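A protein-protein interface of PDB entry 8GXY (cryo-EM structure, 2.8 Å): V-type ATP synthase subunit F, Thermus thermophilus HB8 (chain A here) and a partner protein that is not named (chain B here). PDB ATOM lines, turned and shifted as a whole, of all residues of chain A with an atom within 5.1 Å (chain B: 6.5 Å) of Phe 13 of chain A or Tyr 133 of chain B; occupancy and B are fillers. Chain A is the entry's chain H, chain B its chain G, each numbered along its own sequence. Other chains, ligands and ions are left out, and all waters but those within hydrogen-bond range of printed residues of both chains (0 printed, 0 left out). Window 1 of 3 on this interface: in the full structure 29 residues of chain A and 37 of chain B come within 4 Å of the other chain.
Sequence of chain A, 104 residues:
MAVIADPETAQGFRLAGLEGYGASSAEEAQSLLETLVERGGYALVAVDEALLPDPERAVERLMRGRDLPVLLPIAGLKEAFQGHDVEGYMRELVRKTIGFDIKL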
ATOM      1  N   VAL A   3       6.629 -20.011   1.342  1.00  0.00           N
ATOM      2  CA  VAL A   3       5.954 -20.960   2.219  1.00  0.00           C
ATOM      3  C   VAL A   3       4.732 -20.278   2.817  1.00  0.00           C
ATOM      4  O   VAL A   3       4.851 -19.216   3.437  1.00  0.00           O
ATOM      5  CB  VAL A   3       6.882 -21.470   3.334  1.00  0.00           C
ATOM      6  CG1 VAL A   3       6.210 -22.593   4.112  1.00  0.00           C
ATOM      7  CG2 VAL A   3       8.210 -21.929   2.749  1.00  0.00           C
ATOM      8  N   THR A   9       5.846 -20.828  11.977  1.00  0.00           N
ATOM      9  CA  THR A   9       6.849 -21.296  11.027  1.00  0.00           C
ATOM     10  C   THR A   9       7.042 -20.316   9.878  1.00  0.00           C
ATOM     11  O   THR A   9       8.142 -20.228   9.324  1.00  0.00           O
ATOM     12  CB  THR A   9       6.470 -22.678  10.488  1.00  0.00           C
ATOM     13  OG1 THR A   9       7.626 -23.306   9.917  1.00  0.00           O
ATOM     14  CG2 THR A   9       5.379 -22.577   9.431  1.00  0.00           C
ATOM     15  N   ALA A  10       5.996 -19.577   9.503  1.00  0.00           N
ATOM     16  CA  ALA A  10       6.130 -18.617   8.413  1.00  0.00           C
ATOM     17  C   ALA A  10       7.125 -17.522   8.769  1.00  0.00           C
ATOM     18  O   ALA A  10       7.959 -17.132   7.943  1.00  0.00           O
ATOM     19  CB  ALA A  10       4.768 -18.014   8.076  1.00  0.00           C
ATOM     20  N   GLN A  11       7.053 -17.011   9.997  1.00  0.00           N
ATOM     21  CA  GLN A  11       7.989 -15.978  10.416  1.00  0.00           C
ATOM     22  C   GLN A  11       9.409 -16.517  10.514  1.00  0.00           C
ATOM     23  O   GLN A  11      10.361 -15.802  10.197  1.00  0.00           O
ATOM     24  CB  GLN A  11       7.534 -15.379  11.745  1.00  0.00           C
ATOM     25  CG  GLN A  11       7.614 -16.343  12.909  1.00  0.00           C
ATOM     26  CD  GLN A  11       6.928 -15.816  14.152  1.00  0.00           C
ATOM     27  OE1 GLN A  11       6.236 -14.798  14.112  1.00  0.00           O
ATOM     28  NE2 GLN A  11       7.097 -16.522  15.262  1.00  0.00           N
ATOM     29  N   GLY A  12       9.575 -17.767  10.942  1.00  0.00           N
ATOM     30  CA  GLY A  12      10.901 -18.363  10.922  1.00  0.00           C
ATOM     31  C   GLY A  12      11.447 -18.495   9.513  1.00  0.00           C
ATOM     32  O   GLY A  12      12.623 -18.223   9.260  1.00  0.00           O
ATOM     33  N   PHE A  13      10.597 -18.906   8.574  1.00  0.00           N
ATOM     34  CA  PHE A  13      11.024 -18.968   7.182  1.00  0.00           C
ATOM     35  C   PHE A  13      11.429 -17.590   6.682  1.00  0.00           C
ATOM     36  O   PHE A  13      12.427 -17.447   5.968  1.00  0.00           O
ATOM     37  CB  PHE A  13       9.908 -19.551   6.317  1.00  0.00           C
ATOM     38  CG  PHE A  13      10.089 -21.004   5.989  1.00  0.00           C
ATOM     39  CD1 PHE A  13      11.234 -21.440   5.345  1.00  0.00           C
ATOM     40  CD2 PHE A  13       9.114 -21.931   6.311  1.00  0.00           C
ATOM     41  CE1 PHE A  13      11.408 -22.771   5.034  1.00  0.00           C
ATOM     42  CE2 PHE A  13       9.282 -23.267   6.003  1.00  0.00           C
ATOM     43  CZ  PHE A  13      10.430 -23.686   5.360  1.00  0.00           C
ATOM     44  N   ARG A  14      10.668 -16.561   7.054  1.00  0.00           N
ATOM     45  CA  ARG A  14      11.068 -15.200   6.717  1.00  0.00           C
ATOM     46  C   ARG A  14      12.428 -14.877   7.321  1.00  0.00           C
ATOM     47  O   ARG A  14      13.280 -14.268   6.665  1.00  0.00           O
ATOM     48  CB  ARG A  14      10.010 -14.206   7.198  1.00  0.00           C
ATOM     49  CG  ARG A  14      10.308 -12.745   6.867  1.00  0.00           C
ATOM     50  CD  ARG A  14      10.462 -12.517   5.367  1.00  0.00           C
ATOM     51  NE  ARG A  14       9.209 -12.715   4.648  1.00  0.00           N
ATOM     52  CZ  ARG A  14       8.260 -11.796   4.525  1.00  0.00           C
ATOM     53  NH1 ARG A  14       8.379 -10.599   5.076  1.00  0.00           N
ATOM     54  NH2 ARG A  14       7.163 -12.086   3.832  1.00  0.00           N
ATOM     55  N   LEU A  15      12.648 -15.285   8.570  1.00  0.00           N
ATOM     56  CA  LEU A  15      13.955 -15.141   9.197  1.00  0.00           C
ATOM     57  C   LEU A  15      15.034 -15.882   8.423  1.00  0.00           C
ATOM     58  O   LEU A  15      16.217 -15.550   8.552  1.00  0.00           O
ATOM     59  CB  LEU A  15      13.897 -15.647  10.641  1.00  0.00           C
ATOM     60  CG  LEU A  15      15.220 -15.878  11.376  1.00  0.00           C
ATOM     61  CD1 LEU A  15      15.950 -14.565  11.585  1.00  0.00           C
ATOM     62  CD2 LEU A  15      14.967 -16.568  12.707  1.00  0.00           C
ATOM     63  N   ALA A  16      14.653 -16.883   7.636  1.00  0.00           N
ATOM     64  CA  ALA A  16      15.578 -17.574   6.753  1.00  0.00           C
ATOM     65  C   ALA A  16      15.716 -16.886   5.402  1.00  0.00           C
ATOM     66  O   ALA A  16      16.379 -17.424   4.510  1.00  0.00           O
ATOM     67  CB  ALA A  16      15.134 -19.025   6.551  1.00  0.00           C
ATOM     68  N   GLY A  17      15.109 -15.716   5.230  1.00  0.00           N
ATOM     69  CA  GLY A  17      15.206 -14.983   3.988  1.00  0.00           C
ATOM     70  C   GLY A  17      14.222 -15.403   2.921  1.00  0.00           C
ATOM     71  O   GLY A  17      14.259 -14.848   1.816  1.00  0.00           O
ATOM     72  N   LEU A  18      13.346 -16.356   3.210  1.00  0.00           N
ATOM     73  CA  LEU A  18      12.376 -16.811   2.230  1.00  0.00           C
ATOM     74  C   LEU A  18      11.073 -16.038   2.377  1.00  0.00           C
ATOM     75  O   LEU A  18      10.647 -15.699   3.484  1.00  0.00           O
ATOM     76  CB  LEU A  18      12.109 -18.306   2.399  1.00  0.00           C
ATOM     77  CG  LEU A  18      13.322 -19.231   2.279  1.00  0.00           C
ATOM     78  CD1 LEU A  18      12.873 -20.684   2.309  1.00  0.00           C
ATOM     79  CD2 LEU A  18      14.138 -18.931   1.027  1.00  0.00           C
ATOM     80  N   ILE A  74       3.920 -29.213   3.288  1.00  0.00           N
ATOM     81  CA  ILE A  74       4.916 -29.115   4.345  1.00  0.00           C
ATOM     82  C   ILE A  74       4.284 -29.561   5.653  1.00  0.00           C
ATOM     83  O   ILE A  74       3.076 -29.419   5.867  1.00  0.00           O
ATOM     84  CB  ILE A  74       5.496 -27.686   4.452  1.00  0.00           C
ATOM     85  CG1 ILE A  74       6.973 -27.742   4.847  1.00  0.00           C
ATOM     86  CG2 ILE A  74       4.712 -26.848   5.442  1.00  0.00           C
ATOM     87  CD1 ILE A  74       7.628 -26.378   4.971  1.00  0.00           C
ATOM     88  N   ALA A  75       5.118 -30.107   6.533  1.00  0.00           N
ATOM     89  CA  ALA A  75       4.616 -30.760   7.734  1.00  0.00           C
ATOM     90  C   ALA A  75       3.872 -29.773   8.622  1.00  0.00           C
ATOM     91  O   ALA A  75       4.250 -28.606   8.754  1.00  0.00           O
ATOM     92  CB  ALA A  75       5.769 -31.394   8.513  1.00  0.00           C
ATOM     93  N   ALA B  52      14.330 -36.855   6.639  1.00  0.00           N
ATOM     94  CA  ALA B  52      15.286 -35.792   6.919  1.00  0.00           C
ATOM     95  C   ALA B  52      14.580 -34.454   7.079  1.00  0.00           C
ATOM     96  O   ALA B  52      14.939 -33.650   7.948  1.00  0.00           O
ATOM     97  CB  ALA B  52      16.329 -35.720   5.805  1.00  0.00           C
ATOM     98  N   LEU B  53      13.580 -34.192   6.238  1.00  0.00           N
ATOM     99  CA  LEU B  53      12.813 -32.960   6.366  1.00  0.00           C
ATOM    100  C   LEU B  53      12.109 -32.894   7.710  1.00  0.00           C
ATOM    101  O   LEU B  53      12.046 -31.830   8.331  1.00  0.00           O
ATOM    102  CB  LEU B  53      11.796 -32.850   5.232  1.00  0.00           C
ATOM    103  CG  LEU B  53      11.040 -31.523   5.163  1.00  0.00           C
ATOM    104  CD1 LEU B  53      11.944 -30.410   4.659  1.00  0.00           C
ATOM    105  CD2 LEU B  53       9.812 -31.660   4.282  1.00  0.00           C
ATOM    106  N   ASP B  54      11.557 -34.016   8.168  1.00  0.00           N
ATOM    107  CA  ASP B  54      10.890 -34.030   9.465  1.00  0.00           C
ATOM    108  C   ASP B  54      11.873 -33.718  10.585  1.00  0.00           C
ATOM    109  O   ASP B  54      11.578 -32.921  11.486  1.00  0.00           O
ATOM    110  CB  ASP B  54      10.227 -35.387   9.695  1.00  0.00           C
ATOM    111  CG  ASP B  54       9.538 -35.477  11.042  1.00  0.00           C
ATOM    112  OD1 ASP B  54       8.757 -34.560  11.373  1.00  0.00           O
ATOM    113  OD2 ASP B  54       9.780 -36.462  11.771  1.00  0.00           O
ATOM    114  N   GLN B  55      13.054 -34.335  10.546  1.00  0.00           N
ATOM    115  CA  GLN B  55      14.052 -34.063  11.577  1.00  0.00           C
ATOM    116  C   GLN B  55      14.460 -32.594  11.565  1.00  0.00           C
ATOM    117  O   GLN B  55      14.523 -31.941  12.616  1.00  0.00           O
ATOM    118  CB  GLN B  55      15.272 -34.959  11.376  1.00  0.00           C
ATOM    119  CG  GLN B  55      15.000 -36.434  11.606  1.00  0.00           C
ATOM    120  CD  GLN B  55      16.208 -37.304  11.315  1.00  0.00           C
ATOM    121  OE1 GLN B  55      17.085 -36.928  10.537  1.00  0.00           O
ATOM    122  NE2 GLN B  55      16.260 -38.473  11.941  1.00  0.00           N
ATOM    123  N   ALA B  56      14.735 -32.056  10.377  1.00  0.00           N
ATOM    124  CA  ALA B  56      15.148 -30.662  10.276  1.00  0.00           C
ATOM    125  C   ALA B  56      14.047 -29.726  10.751  1.00  0.00           C
ATOM    126  O   ALA B  56      14.320 -28.726  11.423  1.00  0.00           O
ATOM    127  CB  ALA B  56      15.543 -30.338   8.837  1.00  0.00           C
ATOM    128  N   ALA B  57      12.797 -30.023  10.392  1.00  0.00           N
ATOM    129  CA  ALA B  57      11.681 -29.202  10.841  1.00  0.00           C
ATOM    130  C   ALA B  57      11.579 -29.215  12.354  1.00  0.00           C
ATOM    131  O   ALA B  57      11.394 -28.167  12.981  1.00  0.00           O
ATOM    132  CB  ALA B  57      10.379 -29.708  10.223  1.00  0.00           C
ATOM    133  N   LYS B  58      11.693 -30.394  12.963  1.00  0.00           N
ATOM    134  CA  LYS B  58      11.637 -30.468  14.415  1.00  0.00           C
ATOM    135  C   LYS B  58      12.731 -29.613  15.035  1.00  0.00           C
ATOM    136  O   LYS B  58      12.472 -28.813  15.941  1.00  0.00           O
ATOM    137  CB  LYS B  58      11.759 -31.921  14.872  1.00  0.00           C
ATOM    138  CG  LYS B  58      10.461 -32.707  14.758  1.00  0.00           C
ATOM    139  CD  LYS B  58      10.381 -33.824  15.785  1.00  0.00           C
ATOM    140  CE  LYS B  58      11.615 -34.709  15.744  1.00  0.00           C
ATOM    141  NZ  LYS B  58      11.283 -36.133  16.023  1.00  0.00           N
ATOM    142  N   ALA B  60      14.460 -27.042  13.773  1.00  0.00           N
ATOM    143  CA  ALA B  60      14.329 -25.609  13.536  1.00  0.00           C
ATOM    144  C   ALA B  60      13.173 -25.020  14.331  1.00  0.00           C
ATOM    145  O   ALA B  60      13.286 -23.918  14.880  1.00  0.00           O
ATOM    146  CB  ALA B  60      14.143 -25.340  12.043  1.00  0.00           C
ATOM    147  N   LEU B  64      13.274 -22.113  17.177  1.00  0.00           N
ATOM    148  CA  LEU B  64      12.470 -20.897  17.148  1.00  0.00           C
ATOM    149  C   LEU B  64      11.629 -20.755  18.408  1.00  0.00           C
ATOM    150  O   LEU B  64      11.523 -19.657  18.968  1.00  0.00           O
ATOM    151  CB  LEU B  64      11.570 -20.880  15.918  1.00  0.00           C
ATOM    152  CG  LEU B  64      10.572 -19.717  15.854  1.00  0.00           C
ATOM    153  CD1 LEU B  64      11.285 -18.372  15.932  1.00  0.00           C
ATOM    154  CD2 LEU B  64       9.737 -19.798  14.589  1.00  0.00           C
ATOM    155  N   ALA B  80      12.411 -11.469  13.202  1.00  0.00           N
ATOM    156  CA  ALA B  80      12.285 -12.465  12.143  1.00  0.00           C
ATOM    157  C   ALA B  80      11.626 -11.874  10.906  1.00  0.00           C
ATOM    158  O   ALA B  80      12.085 -12.098   9.781  1.00  0.00           O
ATOM    159  CB  ALA B  80      11.490 -13.667  12.651  1.00  0.00           C
ATOM    160  N   VAL B  83      13.807  -9.586   8.476  1.00  0.00           N
ATOM    161  CA  VAL B  83      14.677 -10.149   7.448  1.00  0.00           C
ATOM    162  C   VAL B  83      13.949 -10.059   6.111  1.00  0.00           C
ATOM    163  O   VAL B  83      12.849 -10.613   5.973  1.00  0.00           O
ATOM    164  CB  VAL B  83      15.065 -11.599   7.775  1.00  0.00           C
ATOM    165  CG1 VAL B  83      15.902 -12.197   6.651  1.00  0.00           C
ATOM    166  CG2 VAL B  83      15.813 -11.664   9.099  1.00  0.00           C
ATOM    167  N   ARG B 128      19.847 -20.158  11.206  1.00  0.00           N
ATOM    168  CA  ARG B 128      20.656 -21.231  10.636  1.00  0.00           C
ATOM    169  C   ARG B 128      19.832 -22.502  10.460  1.00  0.00           C
ATOM    170  O   ARG B 128      19.886 -23.160   9.410  1.00  0.00           O
ATOM    171  CB  ARG B 128      21.867 -21.489  11.536  1.00  0.00           C
ATOM    172  CG  ARG B 128      22.801 -22.598  11.067  1.00  0.00           C
ATOM    173  CD  ARG B 128      23.810 -22.095  10.048  1.00  0.00           C
ATOM    174  NE  ARG B 128      23.255 -22.044   8.701  1.00  0.00           N
ATOM    175  CZ  ARG B 128      23.796 -21.377   7.691  1.00  0.00           C
ATOM    176  NH1 ARG B 128      24.912 -20.683   7.839  1.00  0.00           N
ATOM    177  NH2 ARG B 128      23.203 -21.410   6.501  1.00  0.00           N
ATOM    178  N   ALA B 129      19.063 -22.866  11.486  1.00  0.00           N
ATOM    179  CA  ALA B 129      18.251 -24.073  11.404  1.00  0.00           C
ATOM    180  C   ALA B 129      17.202 -23.955  10.308  1.00  0.00           C
ATOM    181  O   ALA B 129      16.948 -24.918   9.578  1.00  0.00           O
ATOM    182  CB  ALA B 129      17.592 -24.354  12.753  1.00  0.00           C
ATOM    183  N   PHE B 130      16.584 -22.781  10.168  1.00  0.00           N
ATOM    184  CA  PHE B 130      15.594 -22.614   9.111  1.00  0.00           C
ATOM    185  C   PHE B 130      16.234 -22.608   7.730  1.00  0.00           C
ATOM    186  O   PHE B 130      15.609 -23.053   6.764  1.00  0.00           O
ATOM    187  CB  PHE B 130      14.790 -21.335   9.325  1.00  0.00           C
ATOM    188  CG  PHE B 130      13.825 -21.418  10.462  1.00  0.00           C
ATOM    189  CD1 PHE B 130      12.646 -22.128  10.330  1.00  0.00           C
ATOM    190  CD2 PHE B 130      14.093 -20.793  11.664  1.00  0.00           C
ATOM    191  CE1 PHE B 130      11.755 -22.215  11.371  1.00  0.00           C
ATOM    192  CE2 PHE B 130      13.204 -20.874  12.710  1.00  0.00           C
ATOM    193  CZ  PHE B 130      12.031 -21.588  12.564  1.00  0.00           C
ATOM    194  N   ARG B 131      17.465 -22.116   7.605  1.00  0.00           N
ATOM    195  CA  ARG B 131      18.150 -22.217   6.321  1.00  0.00           C
ATOM    196  C   ARG B 131      18.418 -23.676   5.965  1.00  0.00           C
ATOM    197  O   ARG B 131      18.194 -24.100   4.820  1.00  0.00           O
ATOM    198  CB  ARG B 131      19.447 -21.412   6.359  1.00  0.00           C
ATOM    199  CG  ARG B 131      19.224 -19.910   6.237  1.00  0.00           C
ATOM    200  CD  ARG B 131      20.515 -19.124   6.391  1.00  0.00           C
ATOM    201  NE  ARG B 131      20.611 -18.468   7.690  1.00  0.00           N
ATOM    202  CZ  ARG B 131      21.724 -17.940   8.182  1.00  0.00           C
ATOM    203  NH1 ARG B 131      22.862 -17.973   7.508  1.00  0.00           N
ATOM    204  NH2 ARG B 131      21.694 -17.363   9.379  1.00  0.00           N
ATOM    205  N   ARG B 132      18.869 -24.466   6.940  1.00  0.00           N
ATOM    206  CA  ARG B 132      19.034 -25.896   6.693  1.00  0.00           C
ATOM    207  C   ARG B 132      17.701 -26.559   6.356  1.00  0.00           C
ATOM    208  O   ARG B 132      17.647 -27.473   5.524  1.00  0.00           O
ATOM    209  CB  ARG B 132      19.677 -26.565   7.907  1.00  0.00           C
ATOM    210  CG  ARG B 132      21.169 -26.296   8.024  1.00  0.00           C
ATOM    211  CD  ARG B 132      21.916 -27.436   8.699  1.00  0.00           C
ATOM    212  NE  ARG B 132      22.394 -27.065  10.026  1.00  0.00           N
ATOM    213  CZ  ARG B 132      21.708 -27.230  11.150  1.00  0.00           C
ATOM    214  NH1 ARG B 132      20.492 -27.753  11.152  1.00  0.00           N
ATOM    215  NH2 ARG B 132      22.256 -26.859  12.304  1.00  0.00           N
ATOM    216  N   TYR B 133      16.620 -26.114   6.991  1.00  0.00           N
ATOM    217  CA  TYR B 133      15.303 -26.670   6.710  1.00  0.00           C
ATOM    218  C   TYR B 133      14.845 -26.326   5.298  1.00  0.00           C
ATOM    219  O   TYR B 133      14.213 -27.147   4.624  1.00  0.00           O
ATOM    220  CB  TYR B 133      14.314 -26.168   7.760  1.00  0.00           C
ATOM    221  CG  TYR B 133      12.894 -26.640   7.588  1.00  0.00           C
ATOM    222  CD1 TYR B 133      12.591 -27.992   7.567  1.00  0.00           C
ATOM    223  CD2 TYR B 133      11.850 -25.733   7.504  1.00  0.00           C
ATOM    224  CE1 TYR B 133      11.292 -28.426   7.421  1.00  0.00           C
ATOM    225  CE2 TYR B 133      10.547 -26.159   7.370  1.00  0.00           C
ATOM    226  CZ  TYR B 133      10.273 -27.506   7.330  1.00  0.00           C
ATOM    227  OH  TYR B 133       8.974 -27.938   7.192  1.00  0.00           O
ATOM    228  N   ALA B 134      15.154 -25.116   4.832  1.00  0.00           N
ATOM    229  CA  ALA B 134      14.881 -24.765   3.443  1.00  0.00           C
ATOM    230  C   ALA B 134      15.676 -25.650   2.491  1.00  0.00           C
ATOM    231  O   ALA B 134      15.168 -26.071   1.442  1.00  0.00           O
ATOM    232  CB  ALA B 134      15.207 -23.293   3.204  1.00  0.00           C
ATOM    233  N   GLU B 135      16.929 -25.939   2.839  1.00  0.00           N
ATOM    234  CA  GLU B 135      17.723 -26.860   2.030  1.00  0.00           C
ATOM    235  C   GLU B 135      17.073 -28.242   1.966  1.00  0.00           C
ATOM    236  O   GLU B 135      16.996 -28.860   0.892  1.00  0.00           O
ATOM    237  CB  GLU B 135      19.139 -26.934   2.602  1.00  0.00           C
ATOM    238  CG  GLU B 135      20.012 -28.044   2.046  1.00  0.00           C
ATOM    239  CD  GLU B 135      19.947 -29.316   2.875  1.00  0.00           C
ATOM    240  OE1 GLU B 135      19.493 -29.258   4.037  1.00  0.00           O
ATOM    241  OE2 GLU B 135      20.371 -30.374   2.370  1.00  0.00           O
ATOM    242  N   ALA B 136      16.587 -28.737   3.103  1.00  0.00           N
ATOM    243  CA  ALA B 136      15.898 -30.026   3.115  1.00  0.00           C
ATOM    244  C   ALA B 136      14.630 -29.982   2.270  1.00  0.00           C
ATOM    245  O   ALA B 136      14.303 -30.947   1.567  1.00  0.00           O
ATOM    246  CB  ALA B 136      15.567 -30.430   4.551  1.00  0.00           C
ATOM    247  N   LEU B 137      13.898 -28.873   2.338  1.00  0.00           N
ATOM    248  CA  LEU B 137      12.708 -28.709   1.512  1.00  0.00           C
ATOM    249  C   LEU B 137      13.056 -28.788   0.034  1.00  0.00           C
ATOM    250  O   LEU B 137      12.333 -29.413  -0.752  1.00  0.00           O
ATOM    251  CB  LEU B 137      12.044 -27.372   1.831  1.00  0.00           C
ATOM    252  CG  LEU B 137      10.546 -27.250   1.564  1.00  0.00           C
ATOM    253  CD1 LEU B 137       9.749 -28.126   2.517  1.00  0.00           C
ATOM    254  CD2 LEU B 137      10.114 -25.798   1.682  1.00  0.00           C
ATOM    255  N   ILE B 138      14.160 -28.156  -0.367  1.00  0.00           N
ATOM    256  CA  ILE B 138      14.558 -28.196  -1.772  1.00  0.00           C
ATOM    257  C   ILE B 138      14.930 -29.617  -2.181  1.00  0.00           C
ATOM    258  O   ILE B 138      14.625 -30.058  -3.297  1.00  0.00           O
ATOM    259  CB  ILE B 138      15.706 -27.208  -2.029  1.00  0.00           C
ATOM    260  CG1 ILE B 138      15.175 -25.774  -2.007  1.00  0.00           C
ATOM    261  CG2 ILE B 138      16.370 -27.498  -3.364  1.00  0.00           C
ATOM    262  CD1 ILE B 138      16.223 -24.741  -1.656  1.00  0.00           C
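Of the printed residues of chain B, Gln 11 of chain A touches Ala 80. Phe 13 of chain A touches just one residue of chain B: Tyr 133. Of the printed residues of chain B, Leu 15 of chain A touches Ala 80 (3.5 Å) and Val 83 (3.8 Å). Of the printed residues of chain B, Gly 17 of chain A touches Val 83. Printed residues of chain B within 4 Å of Leu 18 of chain A: Ala 134. Asp 54 of chain B touches none of the printed residues of chain A. Gln 55 of chain B touches none of the printed residues of chain A. Printed residues of chain A within 4 Å of Val 83 of chain B: Arg 14 (3.1 Å), Leu 15 (3.8 Å) and Gly 17 (3.9 Å). Tyr 133 of chain B touches just these residues of chain A: Phe 13 and Ile 74. The nearest residue of chain B that does not touch Phe 13 of chain A is Phe 130 of chain B (4.2 Å). The nearest printed residue of chain A that does not touch Ala 134 of chain B is Phe 13 of chain A (4.2 Å).
The backbone carbonyl oxygen of Ala 80 of chain B sits at hydrogen-bond distance from the backbone NH of Leu 15 of chain A.
Hydrophobic or aromatic side chains of chain B that line the printed part of chain A: Ala 80, Val 83, Phe 130, Tyr 133, Ala 134 and Leu 137. Of the 13 printed residues of chain A, 9 touch a printed residue of chain B. Hydrophobic or aromatic side chains of chain A within 4 Å of the printed part of chain B: Phe 13, Leu 15, Ala 16, Leu 18 and Ile 74. Among the printed residues, 12 pairs touch across the chains.
N of Leu 18 of chain A sits at hydrogen-bond distance from O of Phe 13 of chain A, at 3.1 Å.
Among the printed residues, pairs that only touch across the chains: Ile 74 of chain A with Tyr 133 of chain B, Arg 14 of chain A with Val 83 of chain B, Phe 13 of chain A with Tyr 133 of chain B, Gln 11 of chain A with Ala 80 of chain B, Arg 14 of chain A with Ala 80 of chain B, Leu 18 of chain A with Ala 134 of chain B, Gly 12 of chain A with Phe 130 of chain B, Ala 16 of chain A with Phe 130 of chain B, Ile 74 of chain A with Leu 137 of chain B, Leu 15 of chain A with Val 83 of chain B and Gly 17 of chain A with Val 83 of chain B.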
